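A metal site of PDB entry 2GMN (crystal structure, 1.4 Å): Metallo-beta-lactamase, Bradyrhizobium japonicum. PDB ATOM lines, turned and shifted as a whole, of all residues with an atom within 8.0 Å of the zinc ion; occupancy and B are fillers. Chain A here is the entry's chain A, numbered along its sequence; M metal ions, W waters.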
ATOM      1  N   LYS A 137     -22.106 -21.044 -26.012  1.00  0.00           N
ATOM      2  CA  LYS A 137     -22.809 -22.246 -25.575  1.00  0.00           C
ATOM      3  C   LYS A 137     -21.828 -23.222 -24.927  1.00  0.00           C
ATOM      4  O   LYS A 137     -20.623 -23.019 -24.982  1.00  0.00           O
ATOM      5  CB  LYS A 137     -23.535 -22.909 -26.752  1.00  0.00           C
ATOM      6  CG  LYS A 137     -22.712 -23.099 -28.014  1.00  0.00           C
ATOM      7  CD  LYS A 137     -23.102 -22.073 -29.086  1.00  0.00           C
ATOM      8  CE  LYS A 137     -22.013 -21.906 -30.142  1.00  0.00           C
ATOM      9  NZ  LYS A 137     -21.516 -23.195 -30.695  1.00  0.00           N
ATOM     10  N   GLU A 138     -22.371 -24.280 -24.329  1.00  0.00           N
ATOM     11  CA  GLU A 138     -21.557 -25.318 -23.702  1.00  0.00           C
ATOM     12  C   GLU A 138     -20.426 -25.784 -24.616  1.00  0.00           C
ATOM     13  O   GLU A 138     -20.657 -26.142 -25.777  1.00  0.00           O
ATOM     14  CB  GLU A 138     -22.444 -26.512 -23.314  1.00  0.00           C
ATOM     15  CG  GLU A 138     -21.686 -27.783 -22.943  1.00  0.00           C
ATOM     16  CD  GLU A 138     -21.029 -27.701 -21.582  1.00  0.00           C
ATOM     17  OE1 GLU A 138     -21.456 -26.905 -20.723  1.00  0.00           O
ATOM     18  OE2 GLU A 138     -20.083 -28.484 -21.353  1.00  0.00           O
ATOM     19  N   GLY A 139     -19.199 -25.755 -24.089  1.00  0.00           N
ATOM     20  CA  GLY A 139     -18.032 -26.286 -24.787  1.00  0.00           C
ATOM     21  C   GLY A 139     -17.328 -25.325 -25.723  1.00  0.00           C
ATOM     22  O   GLY A 139     -16.277 -25.666 -26.266  1.00  0.00           O
ATOM     23  N   THR A 150     -12.852 -22.396 -21.559  1.00  0.00           N
ATOM     24  CA  THR A 150     -13.949 -23.170 -22.098  1.00  0.00           C
ATOM     25  C   THR A 150     -15.229 -22.834 -21.338  1.00  0.00           C
ATOM     26  O   THR A 150     -15.240 -22.832 -20.117  1.00  0.00           O
ATOM     27  CB  THR A 150     -13.656 -24.679 -22.034  1.00  0.00           C
ATOM     28  OG1 THR A 150     -12.502 -24.944 -22.839  1.00  0.00           O
ATOM     29  CG2 THR A 150     -14.824 -25.514 -22.536  1.00  0.00           C
ATOM     30  N   ALA A 151     -16.286 -22.547 -22.101  1.00  0.00           N
ATOM     31  CA  ALA A 151     -17.581 -22.216 -21.513  1.00  0.00           C
ATOM     32  C   ALA A 151     -18.319 -23.460 -21.075  1.00  0.00           C
ATOM     33  O   ALA A 151     -18.364 -24.465 -21.801  1.00  0.00           O
ATOM     34  CB  ALA A 151     -18.425 -21.451 -22.536  1.00  0.00           C
ATOM     35  N   HIS A 152     -18.895 -23.409 -19.874  1.00  0.00           N
ATOM     36  CA  HIS A 152     -19.782 -24.452 -19.380  1.00  0.00           C
ATOM     37  C   HIS A 152     -21.127 -23.844 -19.013  1.00  0.00           C
ATOM     38  O   HIS A 152     -21.176 -22.893 -18.230  1.00  0.00           O
ATOM     39  CB  HIS A 152     -19.166 -25.159 -18.179  1.00  0.00           C
ATOM     40  CG  HIS A 152     -17.939 -25.941 -18.513  1.00  0.00           C
ATOM     41  ND1 HIS A 152     -17.993 -27.255 -18.948  1.00  0.00           N
ATOM     42  CD2 HIS A 152     -16.624 -25.617 -18.492  1.00  0.00           C
ATOM     43  CE1 HIS A 152     -16.764 -27.695 -19.170  1.00  0.00           C
ATOM     44  NE2 HIS A 152     -15.914 -26.721 -18.907  1.00  0.00           N
ATOM     45  N   ALA A 153     -22.197 -24.379 -19.592  1.00  0.00           N
ATOM     46  CA  ALA A 153     -23.530 -23.858 -19.313  1.00  0.00           C
ATOM     47  C   ALA A 153     -24.005 -24.364 -17.966  1.00  0.00           C
ATOM     48  O   ALA A 153     -24.265 -25.558 -17.787  1.00  0.00           O
ATOM     49  CB  ALA A 153     -24.496 -24.234 -20.430  1.00  0.00           C
ATOM     50  N   THR A 154     -24.122 -23.462 -16.995  1.00  0.00           N
ATOM     51  CA  THR A 154     -24.497 -23.820 -15.630  1.00  0.00           C
ATOM     52  C   THR A 154     -25.620 -22.886 -15.164  1.00  0.00           C
ATOM     53  O   THR A 154     -25.462 -22.150 -14.170  1.00  0.00           O
ATOM     54  CB  THR A 154     -23.284 -23.756 -14.667  1.00  0.00           C
ATOM     55  OG1 THR A 154     -22.619 -22.496 -14.824  1.00  0.00           O
ATOM     56  CG2 THR A 154     -22.287 -24.881 -14.958  1.00  0.00           C
ATOM     57  N   SER A 163     -20.013 -20.921 -16.436  1.00  0.00           N
ATOM     58  CA  SER A 163     -18.811 -21.196 -15.679  1.00  0.00           C
ATOM     59  C   SER A 163     -17.664 -21.410 -16.665  1.00  0.00           C
ATOM     60  O   SER A 163     -17.827 -22.090 -17.677  1.00  0.00           O
ATOM     61  CB  SER A 163     -19.003 -22.441 -14.828  1.00  0.00           C
ATOM     62  OG  SER A 163     -20.011 -22.216 -13.864  1.00  0.00           O
ATOM     63  N   GLU A 165     -13.780 -22.555 -17.604  1.00  0.00           N
ATOM     64  CA  GLU A 165     -12.671 -23.420 -17.215  1.00  0.00           C
ATOM     65  C   GLU A 165     -11.395 -23.070 -17.967  1.00  0.00           C
ATOM     66  O   GLU A 165     -11.428 -22.773 -19.157  1.00  0.00           O
ATOM     67  CB  GLU A 165     -13.048 -24.874 -17.483  1.00  0.00           C
ATOM     68  CG  GLU A 165     -12.006 -25.876 -16.977  1.00  0.00           C
ATOM     69  CD  GLU A 165     -12.539 -27.296 -16.877  1.00  0.00           C
ATOM     70  OE1 GLU A 165     -13.757 -27.487 -16.672  1.00  0.00           O
ATOM     71  OE2 GLU A 165     -11.717 -28.235 -16.969  1.00  0.00           O
ATOM     72  N   LEU A 178     -11.846 -23.309 -12.293  1.00  0.00           N
ATOM     73  CA  LEU A 178     -13.209 -22.995 -12.735  1.00  0.00           C
ATOM     74  C   LEU A 178     -13.655 -21.683 -12.121  1.00  0.00           C
ATOM     75  O   LEU A 178     -13.710 -21.560 -10.901  1.00  0.00           O
ATOM     76  CB  LEU A 178     -14.222 -24.074 -12.344  1.00  0.00           C
ATOM     77  CG  LEU A 178     -15.600 -23.864 -12.980  1.00  0.00           C
ATOM     78  CD1 LEU A 178     -15.589 -24.227 -14.459  1.00  0.00           C
ATOM     79  CD2 LEU A 178     -16.640 -24.634 -12.198  1.00  0.00           C
ATOM     80  N   LYS A 209     -23.973 -31.164 -12.386  1.00  0.00           N
ATOM     81  CA  LYS A 209     -22.850 -30.851 -13.274  1.00  0.00           C
ATOM     82  C   LYS A 209     -21.600 -30.432 -12.497  1.00  0.00           C
ATOM     83  O   LYS A 209     -20.499 -30.949 -12.748  1.00  0.00           O
ATOM     84  CB  LYS A 209     -23.258 -29.743 -14.239  1.00  0.00           C
ATOM     85  CG  LYS A 209     -22.248 -29.471 -15.344  1.00  0.00           C
ATOM     86  CD  LYS A 209     -22.767 -28.389 -16.277  1.00  0.00           C
ATOM     87  CE  LYS A 209     -21.647 -27.834 -17.140  1.00  0.00           C
ATOM     88  NZ  LYS A 209     -21.149 -28.777 -18.165  1.00  0.00           N
ATOM     89  N   MET A 213     -17.497 -32.265 -12.242  1.00  0.00           N
ATOM     90  CA  MET A 213     -16.307 -31.654 -12.832  1.00  0.00           C
ATOM     91  C   MET A 213     -15.061 -31.963 -12.004  1.00  0.00           C
ATOM     92  O   MET A 213     -15.143 -32.173 -10.802  1.00  0.00           O
ATOM     93  CB  MET A 213     -16.494 -30.142 -12.980  1.00  0.00           C
ATOM     94  CG  MET A 213     -17.581 -29.763 -13.966  1.00  0.00           C
ATOM     95  SD  MET A 213     -17.942 -28.009 -13.916  1.00  0.00           S
ATOM     96  CE  MET A 213     -18.621 -27.788 -15.540  1.00  0.00           C
HETATM   97 ZN    ZN M   1     -19.554 -28.543 -19.349  1.00  0.00          ZN
HETATM   98  O   HOH W   1     -18.671 -30.384 -19.273  1.00  0.00           O
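The backbone NH of His 152 is in hydrogen-bond range of the backbone carbonyl oxygen of Ser 163, at 2.8 Å. OE1 of Glu 138 is in hydrogen-bond range of N of Ala 153 (2.9 Å). The side-chain carboxylate of Glu 165 sits at hydrogen-bond distance from a ring nitrogen (NE2) of His 152, at 3.2 Å.
Met 213 touches the zinc ion. Four residues have an atom within 4 Å of the zinc ion: Glu 138, His 152, Lys 209 and Met 213.
The zinc ion is bound by NZ of Lys 209 (2.0 Å), water W1 (2.0 Å), ND1 of His 152 (2.1 Å) and OE2 of Glu 138 (2.1 Å). The zinc ion has four donor atoms within binding distance.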
